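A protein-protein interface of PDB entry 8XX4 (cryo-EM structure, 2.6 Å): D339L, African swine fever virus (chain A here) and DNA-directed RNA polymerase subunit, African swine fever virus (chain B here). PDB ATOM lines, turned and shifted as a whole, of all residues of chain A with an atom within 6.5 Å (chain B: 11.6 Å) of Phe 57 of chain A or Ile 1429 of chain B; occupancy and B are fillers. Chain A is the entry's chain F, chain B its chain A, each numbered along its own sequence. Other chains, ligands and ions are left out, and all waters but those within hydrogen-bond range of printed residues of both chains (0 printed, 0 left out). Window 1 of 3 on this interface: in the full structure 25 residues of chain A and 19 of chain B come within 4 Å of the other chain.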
ATOM      1  N   ILE A  12     -23.107   8.330   9.342  1.00  0.00           N
ATOM      2  CA  ILE A  12     -22.166   8.942  10.265  1.00  0.00           C
ATOM      3  C   ILE A  12     -20.915   8.082  10.286  1.00  0.00           C
ATOM      4  O   ILE A  12     -20.904   7.000  10.884  1.00  0.00           O
ATOM      5  CB  ILE A  12     -22.764   9.096  11.664  1.00  0.00           C
ATOM      6  CG1 ILE A  12     -23.976  10.021  11.606  1.00  0.00           C
ATOM      7  CG2 ILE A  12     -21.739   9.645  12.597  1.00  0.00           C
ATOM      8  CD1 ILE A  12     -25.007   9.724  12.639  1.00  0.00           C
ATOM      9  N   SER A  54     -33.215  10.804  15.366  1.00  0.00           N
ATOM     10  CA  SER A  54     -33.129   9.485  15.968  1.00  0.00           C
ATOM     11  C   SER A  54     -31.833   9.384  16.746  1.00  0.00           C
ATOM     12  O   SER A  54     -30.917  10.191  16.552  1.00  0.00           O
ATOM     13  CB  SER A  54     -33.173   8.389  14.898  1.00  0.00           C
ATOM     14  OG  SER A  54     -31.865   7.977  14.547  1.00  0.00           O
ATOM     15  N   PRO A  55     -31.730   8.422  17.657  1.00  0.00           N
ATOM     16  CA  PRO A  55     -30.419   8.090  18.212  1.00  0.00           C
ATOM     17  C   PRO A  55     -29.489   7.614  17.107  1.00  0.00           C
ATOM     18  O   PRO A  55     -29.924   7.109  16.073  1.00  0.00           O
ATOM     19  CB  PRO A  55     -30.727   6.971  19.209  1.00  0.00           C
ATOM     20  CG  PRO A  55     -32.152   7.157  19.548  1.00  0.00           C
ATOM     21  CD  PRO A  55     -32.814   7.690  18.327  1.00  0.00           C
ATOM     22  N   CYS A  56     -28.193   7.810  17.320  1.00  0.00           N
ATOM     23  CA  CYS A  56     -27.222   7.374  16.329  1.00  0.00           C
ATOM     24  C   CYS A  56     -27.067   5.862  16.387  1.00  0.00           C
ATOM     25  O   CYS A  56     -26.183   5.350  17.078  1.00  0.00           O
ATOM     26  CB  CYS A  56     -25.875   8.066  16.545  1.00  0.00           C
ATOM     27  SG  CYS A  56     -24.563   7.521  15.434  1.00  0.00           S
ATOM     28  N   PHE A  57     -27.932   5.143  15.680  1.00  0.00           N
ATOM     29  CA  PHE A  57     -27.849   3.691  15.652  1.00  0.00           C
ATOM     30  C   PHE A  57     -26.578   3.247  14.948  1.00  0.00           C
ATOM     31  O   PHE A  57     -26.209   3.792  13.910  1.00  0.00           O
ATOM     32  CB  PHE A  57     -29.052   3.097  14.930  1.00  0.00           C
ATOM     33  CG  PHE A  57     -30.368   3.618  15.401  1.00  0.00           C
ATOM     34  CD1 PHE A  57     -30.887   3.223  16.613  1.00  0.00           C
ATOM     35  CD2 PHE A  57     -31.101   4.484  14.620  1.00  0.00           C
ATOM     36  CE1 PHE A  57     -32.099   3.693  17.042  1.00  0.00           C
ATOM     37  CE2 PHE A  57     -32.316   4.953  15.046  1.00  0.00           C
ATOM     38  CZ  PHE A  57     -32.814   4.558  16.261  1.00  0.00           C
ATOM     39  N   ILE A  58     -25.919   2.249  15.504  1.00  0.00           N
ATOM     40  CA  ILE A  58     -24.747   1.668  14.864  1.00  0.00           C
ATOM     41  C   ILE A  58     -25.201   0.745  13.747  1.00  0.00           C
ATOM     42  O   ILE A  58     -26.144  -0.036  13.913  1.00  0.00           O
ATOM     43  CB  ILE A  58     -23.882   0.925  15.895  1.00  0.00           C
ATOM     44  CG1 ILE A  58     -23.337   1.906  16.927  1.00  0.00           C
ATOM     45  CG2 ILE A  58     -22.741   0.205  15.213  1.00  0.00           C
ATOM     46  CD1 ILE A  58     -22.829   3.176  16.326  1.00  0.00           C
ATOM     47  N   MET A  59     -24.544   0.845  12.594  1.00  0.00           N
ATOM     48  CA  MET A  59     -24.882  -0.006  11.462  1.00  0.00           C
ATOM     49  C   MET A  59     -24.740  -1.470  11.848  1.00  0.00           C
ATOM     50  O   MET A  59     -23.748  -1.872  12.460  1.00  0.00           O
ATOM     51  CB  MET A  59     -23.985   0.321  10.274  1.00  0.00           C
ATOM     52  CG  MET A  59     -24.293   1.646   9.631  1.00  0.00           C
ATOM     53  SD  MET A  59     -23.239   1.999   8.222  1.00  0.00           S
ATOM     54  CE  MET A  59     -23.955   3.534   7.662  1.00  0.00           C
ATOM     55  N   ARG A  66     -19.899   2.165  11.763  1.00  0.00           N
ATOM     56  CA  ARG A  66     -20.489   3.471  11.531  1.00  0.00           C
ATOM     57  C   ARG A  66     -21.927   3.513  12.034  1.00  0.00           C
ATOM     58  O   ARG A  66     -22.565   2.488  12.271  1.00  0.00           O
ATOM     59  CB  ARG A  66     -20.443   3.815  10.046  1.00  0.00           C
ATOM     60  CG  ARG A  66     -19.063   4.109   9.518  1.00  0.00           C
ATOM     61  CD  ARG A  66     -18.911   3.597   8.106  1.00  0.00           C
ATOM     62  NE  ARG A  66     -19.776   4.295   7.163  1.00  0.00           N
ATOM     63  CZ  ARG A  66     -20.374   3.717   6.130  1.00  0.00           C
ATOM     64  NH1 ARG A  66     -20.237   2.425   5.886  1.00  0.00           N
ATOM     65  NH2 ARG A  66     -21.126   4.456   5.321  1.00  0.00           N
ATOM     66  N   GLY A  67     -22.437   4.729  12.196  1.00  0.00           N
ATOM     67  CA  GLY A  67     -23.813   4.936  12.593  1.00  0.00           C
ATOM     68  C   GLY A  67     -24.581   5.642  11.502  1.00  0.00           C
ATOM     69  O   GLY A  67     -23.959   6.156  10.571  1.00  0.00           O
ATOM     70  N   TYR A  68     -25.913   5.672  11.560  1.00  0.00           N
ATOM     71  CA  TYR A  68     -26.655   6.358  10.508  1.00  0.00           C
ATOM     72  C   TYR A  68     -27.486   7.530  11.010  1.00  0.00           C
ATOM     73  O   TYR A  68     -27.296   8.645  10.516  1.00  0.00           O
ATOM     74  CB  TYR A  68     -27.524   5.382   9.702  1.00  0.00           C
ATOM     75  CG  TYR A  68     -28.254   4.297  10.452  1.00  0.00           C
ATOM     76  CD1 TYR A  68     -27.587   3.174  10.917  1.00  0.00           C
ATOM     77  CD2 TYR A  68     -29.622   4.362  10.628  1.00  0.00           C
ATOM     78  CE1 TYR A  68     -28.258   2.174  11.569  1.00  0.00           C
ATOM     79  CE2 TYR A  68     -30.297   3.366  11.277  1.00  0.00           C
ATOM     80  CZ  TYR A  68     -29.611   2.274  11.743  1.00  0.00           C
ATOM     81  OH  TYR A  68     -30.287   1.277  12.396  1.00  0.00           O
ATOM     82  N   MET A  69     -28.400   7.328  11.961  1.00  0.00           N
ATOM     83  CA  MET A  69     -29.323   8.371  12.412  1.00  0.00           C
ATOM     84  C   MET A  69     -30.319   8.806  11.342  1.00  0.00           C
ATOM     85  O   MET A  69     -29.932   9.220  10.248  1.00  0.00           O
ATOM     86  CB  MET A  69     -28.571   9.609  12.917  1.00  0.00           C
ATOM     87  CG  MET A  69     -29.440  10.602  13.661  1.00  0.00           C
ATOM     88  SD  MET A  69     -28.516  12.012  14.275  1.00  0.00           S
ATOM     89  CE  MET A  69     -27.605  11.263  15.612  1.00  0.00           C
ATOM     90  N   HIS A  70     -31.606   8.724  11.663  1.00  0.00           N
ATOM     91  CA  HIS A  70     -32.658   9.316  10.851  1.00  0.00           C
ATOM     92  C   HIS A  70     -32.944  10.723  11.349  1.00  0.00           C
ATOM     93  O   HIS A  70     -33.019  10.958  12.556  1.00  0.00           O
ATOM     94  CB  HIS A  70     -33.937   8.486  10.920  1.00  0.00           C
ATOM     95  CG  HIS A  70     -33.712   7.012  10.841  1.00  0.00           C
ATOM     96  ND1 HIS A  70     -33.378   6.373   9.669  1.00  0.00           N
ATOM     97  CD2 HIS A  70     -33.785   6.049  11.787  1.00  0.00           C
ATOM     98  CE1 HIS A  70     -33.250   5.081   9.897  1.00  0.00           C
ATOM     99  NE2 HIS A  70     -33.492   4.857  11.174  1.00  0.00           N
ATOM    100  N   GLY B   4     -28.829   6.930   2.346  1.00  0.00           N
ATOM    101  CA  GLY B   4     -28.693   6.591   3.745  1.00  0.00           C
ATOM    102  C   GLY B   4     -28.759   5.099   3.994  1.00  0.00           C
ATOM    103  O   GLY B   4     -29.215   4.315   3.168  1.00  0.00           O
ATOM    104  N   TYR B   5     -28.286   4.708   5.173  1.00  0.00           N
ATOM    105  CA  TYR B   5     -28.298   3.304   5.552  1.00  0.00           C
ATOM    106  C   TYR B   5     -29.727   2.818   5.734  1.00  0.00           C
ATOM    107  O   TYR B   5     -30.525   3.445   6.433  1.00  0.00           O
ATOM    108  CB  TYR B   5     -27.505   3.105   6.840  1.00  0.00           C
ATOM    109  CG  TYR B   5     -27.510   1.688   7.359  1.00  0.00           C
ATOM    110  CD1 TYR B   5     -26.552   0.777   6.949  1.00  0.00           C
ATOM    111  CD2 TYR B   5     -28.470   1.264   8.262  1.00  0.00           C
ATOM    112  CE1 TYR B   5     -26.552  -0.511   7.426  1.00  0.00           C
ATOM    113  CE2 TYR B   5     -28.476  -0.020   8.738  1.00  0.00           C
ATOM    114  CZ  TYR B   5     -27.516  -0.901   8.320  1.00  0.00           C
ATOM    115  OH  TYR B   5     -27.524  -2.185   8.798  1.00  0.00           O
ATOM    116  N   ALA B   6     -30.043   1.685   5.116  1.00  0.00           N
ATOM    117  CA  ALA B   6     -31.375   1.118   5.202  1.00  0.00           C
ATOM    118  C   ALA B   6     -31.270  -0.388   5.368  1.00  0.00           C
ATOM    119  O   ALA B   6     -30.259  -1.003   5.026  1.00  0.00           O
ATOM    120  CB  ALA B   6     -32.217   1.458   3.968  1.00  0.00           C
ATOM    121  N   GLU B   7     -32.327  -0.970   5.918  1.00  0.00           N
ATOM    122  CA  GLU B   7     -32.461  -2.410   6.042  1.00  0.00           C
ATOM    123  C   GLU B   7     -33.818  -2.818   5.502  1.00  0.00           C
ATOM    124  O   GLU B   7     -34.798  -2.086   5.638  1.00  0.00           O
ATOM    125  CB  GLU B   7     -32.316  -2.867   7.494  1.00  0.00           C
ATOM    126  CG  GLU B   7     -30.893  -3.153   7.915  1.00  0.00           C
ATOM    127  CD  GLU B   7     -30.762  -3.355   9.407  1.00  0.00           C
ATOM    128  OE1 GLU B   7     -31.746  -3.791  10.034  1.00  0.00           O
ATOM    129  OE2 GLU B   7     -29.677  -3.071   9.954  1.00  0.00           O
ATOM    130  N   MET B 472     -14.246  -6.458  14.527  1.00  0.00           N
ATOM    131  CA  MET B 472     -15.499  -6.963  15.078  1.00  0.00           C
ATOM    132  C   MET B 472     -15.485  -8.486  15.157  1.00  0.00           C
ATOM    133  O   MET B 472     -15.838  -9.078  16.188  1.00  0.00           O
ATOM    134  CB  MET B 472     -16.661  -6.485  14.212  1.00  0.00           C
ATOM    135  CG  MET B 472     -17.031  -5.030  14.395  1.00  0.00           C
ATOM    136  SD  MET B 472     -18.792  -4.749  14.186  1.00  0.00           S
ATOM    137  CE  MET B 472     -18.928  -3.068  14.754  1.00  0.00           C
ATOM    138  N   VAL B 475     -13.042  -9.607  17.876  1.00  0.00           N
ATOM    139  CA  VAL B 475     -13.622  -9.418  19.201  1.00  0.00           C
ATOM    140  C   VAL B 475     -14.582 -10.551  19.512  1.00  0.00           C
ATOM    141  O   VAL B 475     -14.535 -11.159  20.587  1.00  0.00           O
ATOM    142  CB  VAL B 475     -14.337  -8.059  19.289  1.00  0.00           C
ATOM    143  CG1 VAL B 475     -15.384  -8.097  20.382  1.00  0.00           C
ATOM    144  CG2 VAL B 475     -13.356  -6.951  19.539  1.00  0.00           C
ATOM    145  N   GLU B 476     -15.458 -10.859  18.568  1.00  0.00           N
ATOM    146  CA  GLU B 476     -16.483 -11.854  18.833  1.00  0.00           C
ATOM    147  C   GLU B 476     -15.936 -13.275  18.812  1.00  0.00           C
ATOM    148  O   GLU B 476     -16.438 -14.137  19.540  1.00  0.00           O
ATOM    149  CB  GLU B 476     -17.606 -11.675  17.832  1.00  0.00           C
ATOM    150  CG  GLU B 476     -18.367 -12.895  17.534  1.00  0.00           C
ATOM    151  CD  GLU B 476     -18.992 -12.775  16.204  1.00  0.00           C
ATOM    152  OE1 GLU B 476     -19.781 -11.831  16.043  1.00  0.00           O
ATOM    153  OE2 GLU B 476     -18.674 -13.589  15.321  1.00  0.00           O
ATOM    154  N   TYR B 840     -36.728 -10.867  24.217  1.00  0.00           N
ATOM    155  CA  TYR B 840     -36.344 -10.137  25.419  1.00  0.00           C
ATOM    156  C   TYR B 840     -37.114 -10.570  26.656  1.00  0.00           C
ATOM    157  O   TYR B 840     -36.730 -10.202  27.769  1.00  0.00           O
ATOM    158  CB  TYR B 840     -36.527  -8.640  25.202  1.00  0.00           C
ATOM    159  CG  TYR B 840     -35.532  -8.069  24.239  1.00  0.00           C
ATOM    160  CD1 TYR B 840     -34.175  -8.215  24.455  1.00  0.00           C
ATOM    161  CD2 TYR B 840     -35.946  -7.393  23.107  1.00  0.00           C
ATOM    162  CE1 TYR B 840     -33.262  -7.701  23.577  1.00  0.00           C
ATOM    163  CE2 TYR B 840     -35.039  -6.877  22.226  1.00  0.00           C
ATOM    164  CZ  TYR B 840     -33.700  -7.033  22.465  1.00  0.00           C
ATOM    165  OH  TYR B 840     -32.792  -6.515  21.585  1.00  0.00           O
ATOM    166  N   TYR B1037     -30.863 -13.407  25.282  1.00  0.00           N
ATOM    167  CA  TYR B1037     -31.757 -12.834  24.290  1.00  0.00           C
ATOM    168  C   TYR B1037     -31.163 -13.008  22.901  1.00  0.00           C
ATOM    169  O   TYR B1037     -29.982 -12.732  22.683  1.00  0.00           O
ATOM    170  CB  TYR B1037     -31.984 -11.352  24.575  1.00  0.00           C
ATOM    171  CG  TYR B1037     -32.471 -11.050  25.967  1.00  0.00           C
ATOM    172  CD1 TYR B1037     -33.439 -11.833  26.567  1.00  0.00           C
ATOM    173  CD2 TYR B1037     -31.967  -9.973  26.679  1.00  0.00           C
ATOM    174  CE1 TYR B1037     -33.891 -11.553  27.832  1.00  0.00           C
ATOM    175  CE2 TYR B1037     -32.411  -9.689  27.948  1.00  0.00           C
ATOM    176  CZ  TYR B1037     -33.374 -10.484  28.517  1.00  0.00           C
ATOM    177  OH  TYR B1037     -33.829 -10.214  29.781  1.00  0.00           O
ATOM    178  N   ARG B1421     -31.005 -10.972  12.360  1.00  0.00           N
ATOM    179  CA  ARG B1421     -30.996 -10.156  13.571  1.00  0.00           C
ATOM    180  C   ARG B1421     -31.141 -11.100  14.766  1.00  0.00           C
ATOM    181  O   ARG B1421     -32.185 -11.219  15.408  1.00  0.00           O
ATOM    182  CB  ARG B1421     -32.094  -9.101  13.512  1.00  0.00           C
ATOM    183  CG  ARG B1421     -32.391  -8.386  14.820  1.00  0.00           C
ATOM    184  CD  ARG B1421     -33.489  -7.359  14.664  1.00  0.00           C
ATOM    185  NE  ARG B1421     -33.537  -6.791  13.323  1.00  0.00           N
ATOM    186  CZ  ARG B1421     -33.076  -5.590  13.005  1.00  0.00           C
ATOM    187  NH1 ARG B1421     -32.522  -4.800  13.911  1.00  0.00           N
ATOM    188  NH2 ARG B1421     -33.178  -5.168  11.749  1.00  0.00           N
ATOM    189  N   ILE B1422     -30.065 -11.845  15.015  1.00  0.00           N
ATOM    190  CA  ILE B1422     -29.961 -12.750  16.150  1.00  0.00           C
ATOM    191  C   ILE B1422     -28.547 -12.656  16.701  1.00  0.00           C
ATOM    192  O   ILE B1422     -27.659 -12.057  16.096  1.00  0.00           O
ATOM    193  CB  ILE B1422     -30.273 -14.216  15.790  1.00  0.00           C
ATOM    194  CG1 ILE B1422     -29.069 -14.838  15.098  1.00  0.00           C
ATOM    195  CG2 ILE B1422     -31.509 -14.335  14.920  1.00  0.00           C
ATOM    196  CD1 ILE B1422     -29.014 -16.296  15.246  1.00  0.00           C
ATOM    197  N   GLY B1423     -28.342 -13.277  17.854  1.00  0.00           N
ATOM    198  CA  GLY B1423     -27.002 -13.365  18.402  1.00  0.00           C
ATOM    199  C   GLY B1423     -26.483 -12.005  18.804  1.00  0.00           C
ATOM    200  O   GLY B1423     -27.173 -11.228  19.468  1.00  0.00           O
ATOM    201  N   THR B1424     -25.250 -11.703  18.397  1.00  0.00           N
ATOM    202  CA  THR B1424     -24.636 -10.432  18.761  1.00  0.00           C
ATOM    203  C   THR B1424     -25.374  -9.245  18.170  1.00  0.00           C
ATOM    204  O   THR B1424     -25.183  -8.118  18.630  1.00  0.00           O
ATOM    205  CB  THR B1424     -23.173 -10.395  18.319  1.00  0.00           C
ATOM    206  OG1 THR B1424     -23.071 -10.835  16.963  1.00  0.00           O
ATOM    207  CG2 THR B1424     -22.331 -11.291  19.197  1.00  0.00           C
ATOM    208  N   MET B1425     -26.221  -9.469  17.172  1.00  0.00           N
ATOM    209  CA  MET B1425     -26.950  -8.395  16.516  1.00  0.00           C
ATOM    210  C   MET B1425     -28.443  -8.436  16.808  1.00  0.00           C
ATOM    211  O   MET B1425     -29.233  -7.860  16.059  1.00  0.00           O
ATOM    212  CB  MET B1425     -26.679  -8.444  15.018  1.00  0.00           C
ATOM    213  CG  MET B1425     -25.242  -8.089  14.678  1.00  0.00           C
ATOM    214  SD  MET B1425     -24.879  -8.345  12.949  1.00  0.00           S
ATOM    215  CE  MET B1425     -26.397  -9.143  12.463  1.00  0.00           C
ATOM    216  N   TYR B1426     -28.844  -9.106  17.888  1.00  0.00           N
ATOM    217  CA  TYR B1426     -30.240  -9.067  18.301  1.00  0.00           C
ATOM    218  C   TYR B1426     -30.608  -7.703  18.865  1.00  0.00           C
ATOM    219  O   TYR B1426     -31.640  -7.131  18.500  1.00  0.00           O
ATOM    220  CB  TYR B1426     -30.513 -10.161  19.329  1.00  0.00           C
ATOM    221  CG  TYR B1426     -31.978 -10.395  19.566  1.00  0.00           C
ATOM    222  CD1 TYR B1426     -32.785 -10.893  18.562  1.00  0.00           C
ATOM    223  CD2 TYR B1426     -32.557 -10.118  20.793  1.00  0.00           C
ATOM    224  CE1 TYR B1426     -34.119 -11.106  18.767  1.00  0.00           C
ATOM    225  CE2 TYR B1426     -33.895 -10.330  21.007  1.00  0.00           C
ATOM    226  CZ  TYR B1426     -34.671 -10.823  19.989  1.00  0.00           C
ATOM    227  OH  TYR B1426     -36.009 -11.040  20.179  1.00  0.00           O
ATOM    228  N   SER B1427     -29.778  -7.169  19.752  1.00  0.00           N
ATOM    229  CA  SER B1427     -29.970  -5.842  20.316  1.00  0.00           C
ATOM    230  C   SER B1427     -29.126  -4.856  19.533  1.00  0.00           C
ATOM    231  O   SER B1427     -27.966  -5.141  19.220  1.00  0.00           O
ATOM    232  CB  SER B1427     -29.585  -5.806  21.794  1.00  0.00           C
ATOM    233  OG  SER B1427     -30.380  -6.692  22.555  1.00  0.00           O
ATOM    234  N   ASP B1428     -29.704  -3.711  19.205  1.00  0.00           N
ATOM    235  CA  ASP B1428     -28.971  -2.715  18.450  1.00  0.00           C
ATOM    236  C   ASP B1428     -28.330  -1.705  19.387  1.00  0.00           C
ATOM    237  O   ASP B1428     -28.889  -1.340  20.422  1.00  0.00           O
ATOM    238  CB  ASP B1428     -29.876  -2.010  17.445  1.00  0.00           C
ATOM    239  CG  ASP B1428     -31.232  -1.703  18.003  1.00  0.00           C
ATOM    240  OD1 ASP B1428     -31.942  -2.651  18.400  1.00  0.00           O
ATOM    241  OD2 ASP B1428     -31.596  -0.512  18.023  1.00  0.00           O
ATOM    242  N   ILE B1429     -27.136  -1.269  19.012  1.00  0.00           N
ATOM    243  CA  ILE B1429     -26.330  -0.362  19.813  1.00  0.00           C
ATOM    244  C   ILE B1429     -26.554   1.052  19.313  1.00  0.00           C
ATOM    245  O   ILE B1429     -26.528   1.304  18.105  1.00  0.00           O
ATOM    246  CB  ILE B1429     -24.842  -0.739  19.746  1.00  0.00           C
ATOM    247  CG1 ILE B1429     -24.664  -2.228  20.019  1.00  0.00           C
ATOM    248  CG2 ILE B1429     -24.041   0.082  20.724  1.00  0.00           C
ATOM    249  CD1 ILE B1429     -25.238  -2.681  21.335  1.00  0.00           C
ATOM    250  N   ILE B1430     -26.793   1.969  20.239  1.00  0.00           N
ATOM    251  CA  ILE B1430     -26.854   3.385  19.934  1.00  0.00           C
ATOM    252  C   ILE B1430     -25.747   4.074  20.715  1.00  0.00           C
ATOM    253  O   ILE B1430     -25.258   3.570  21.726  1.00  0.00           O
ATOM    254  CB  ILE B1430     -28.233   3.991  20.258  1.00  0.00           C
ATOM    255  CG1 ILE B1430     -28.380   4.218  21.756  1.00  0.00           C
ATOM    256  CG2 ILE B1430     -29.333   3.076  19.779  1.00  0.00           C
ATOM    257  CD1 ILE B1430     -29.724   4.749  22.157  1.00  0.00           C
ATOM    258  N   MET B1431     -25.335   5.235  20.224  1.00  0.00           N
ATOM    259  CA  MET B1431     -24.234   5.979  20.817  1.00  0.00           C
ATOM    260  C   MET B1431     -24.752   6.799  21.988  1.00  0.00           C
ATOM    261  O   MET B1431     -25.831   7.395  21.905  1.00  0.00           O
ATOM    262  CB  MET B1431     -23.568   6.887  19.783  1.00  0.00           C
ATOM    263  CG  MET B1431     -23.127   6.177  18.522  1.00  0.00           C
ATOM    264  SD  MET B1431     -21.505   5.399  18.597  1.00  0.00           S
ATOM    265  CE  MET B1431     -20.666   6.394  19.806  1.00  0.00           C
ATOM    266  N   ASP B1432     -23.989   6.818  23.079  1.00  0.00           N
ATOM    267  CA  ASP B1432     -24.366   7.576  24.265  1.00  0.00           C
ATOM    268  C   ASP B1432     -24.030   9.049  24.089  1.00  0.00           C
ATOM    269  O   ASP B1432     -22.932   9.485  24.440  1.00  0.00           O
ATOM    270  CB  ASP B1432     -23.666   7.016  25.499  1.00  0.00           C
ATOM    271  CG  ASP B1432     -24.453   7.236  26.764  1.00  0.00           C
ATOM    272  OD1 ASP B1432     -25.352   8.100  26.768  1.00  0.00           O
ATOM    273  OD2 ASP B1432     -24.174   6.542  27.759  1.00  0.00           O
ATOM    274  N   GLU B1433     -24.977   9.824  23.562  1.00  0.00           N
ATOM    275  CA  GLU B1433     -24.699  11.216  23.228  1.00  0.00           C
ATOM    276  C   GLU B1433     -24.359  12.038  24.463  1.00  0.00           C
ATOM    277  O   GLU B1433     -23.437  12.860  24.432  1.00  0.00           O
ATOM    278  CB  GLU B1433     -25.888  11.822  22.492  1.00  0.00           C
ATOM    279  CG  GLU B1433     -25.899  11.508  21.015  1.00  0.00           C
ATOM    280  CD  GLU B1433     -27.237  11.004  20.534  1.00  0.00           C
ATOM    281  OE1 GLU B1433     -28.227  11.134  21.281  1.00  0.00           O
ATOM    282  OE2 GLU B1433     -27.302  10.481  19.403  1.00  0.00           O
ATOM    283  N   ILE B1436     -20.789  11.006  25.687  1.00  0.00           N
ATOM    284  CA  ILE B1436     -19.726  11.453  24.795  1.00  0.00           C
ATOM    285  C   ILE B1436     -19.587  12.967  24.847  1.00  0.00           C
ATOM    286  O   ILE B1436     -18.474  13.503  24.809  1.00  0.00           O
ATOM    287  CB  ILE B1436     -19.985  10.955  23.365  1.00  0.00           C
ATOM    288  CG1 ILE B1436     -19.969   9.432  23.330  1.00  0.00           C
ATOM    289  CG2 ILE B1436     -18.934  11.477  22.420  1.00  0.00           C
ATOM    290  CD1 ILE B1436     -20.774   8.861  22.214  1.00  0.00           C
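O of Ile 1429 of chain B lies within hydrogen-bond range of N of Ile 58 of chain A (2.8 Å). O of Cys 56 of chain A sits at hydrogen-bond distance from N of Met 1431 of chain B, at 3.3 Å.
The side-chain hydroxyl (OH) of Tyr 5 of chain B is in hydrogen-bond range of the side-chain carboxylate (OE2) of Glu 7 of chain B (2.6 Å). The backbone carbonyl oxygen (O) of Phe 57 of chain A is in hydrogen-bond range of the backbone NH (N) of Tyr 68 of chain A, 3.0 Å away. The backbone NH of Met 59 of chain A is in hydrogen-bond range of the backbone carbonyl oxygen of Arg 66 of chain A, 2.6 Å away.
Among the printed residues, pairs that only touch across the chains: Tyr 68 of chain A with Tyr 5 of chain B, Ile 58 of chain A with Met 1431 of chain B, Cys 56 of chain A with Glu 1433 of chain B, Phe 57 of chain A with Ile 1430 of chain B, Cys 56 of chain A with Ile 1430 of chain B, Met 59 of chain A with Tyr 5 of chain B, Phe 57 of chain A with Ile 1429 of chain B, Pro 55 of chain A with Ile 1430 of chain B and Met 69 of chain A with Glu 1433 of chain B.
Of the printed residues of chain B, Phe 57 of chain A touches Ile 1429 (3.7 Å) and Ile 1430 (3.5 Å). Ile 1429 of chain B touches two residues of chain A. No residue of chain B comes within 4 Å of Ser 54 of chain A. Of chain B, only Ile 1430 comes within 4 Å of Pro 55 of chain A. Printed residues of chain B within 4 Å of Cys 56 of chain A: Ile 1430, Met 1431 and Glu 1433. Ile 58 of chain A touches two residues of chain B. Met 59 of chain A touches just one residue of chain B: Tyr 5 (3.6 Å). Printed residues of chain B within 4 Å of Tyr 68 of chain A: Tyr 5 (3.4 Å). Met 69 of chain A touches one residue of chain B. No residue of chain B comes within 4 Å of His 70 of chain A. Printed residues of chain A within 4 Å of Glu 1433 of chain B: Cys 56 (3.5 Å) and Met 69 (3.9 Å). Of the printed residues of chain A, Ile 1430 of chain B touches Pro 55, Cys 56 and Phe 57. Printed residues of chain A within 4 Å of Tyr 5 of chain B: Met 59 (3.6 Å) and Tyr 68 (3.4 Å). Met 1425 of chain B touches none of the printed residues of chain A. The nearest residue of chain A that does not touch Ile 1429 of chain B is Cys 56 of chain A (4.2 Å). The nearest printed residue of chain A that does not touch Ile 1430 of chain B is Ile 58 of chain A (4.7 Å).
Of the 23 printed residues of chain B, 5 touch a printed residue of chain A. Printed residues of chain B that touch a printed residue of chain A: Tyr 5, Ile 1429, Ile 1430, Met 1431 and Glu 1433. Hydrophobic or aromatic side chains of chain B that line the printed part of chain A: Tyr 5, Ile 1430 and Met 1431. Printed residues of chain A that touch a printed residue of chain B: Pro 55, Cys 56, Phe 57, Ile 58, Met 59, Tyr 68 and Met 69. Hydrophobic or aromatic side chains of chain A that line the printed part of chain B: Pro 55, Phe 57, Ile 58, Met 59, Tyr 68 and Met 69. Along chain A the printed residues that touch a printed residue of chain B span positions 55 to 69. Among the printed residues, 11 pairs touch across the chains.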
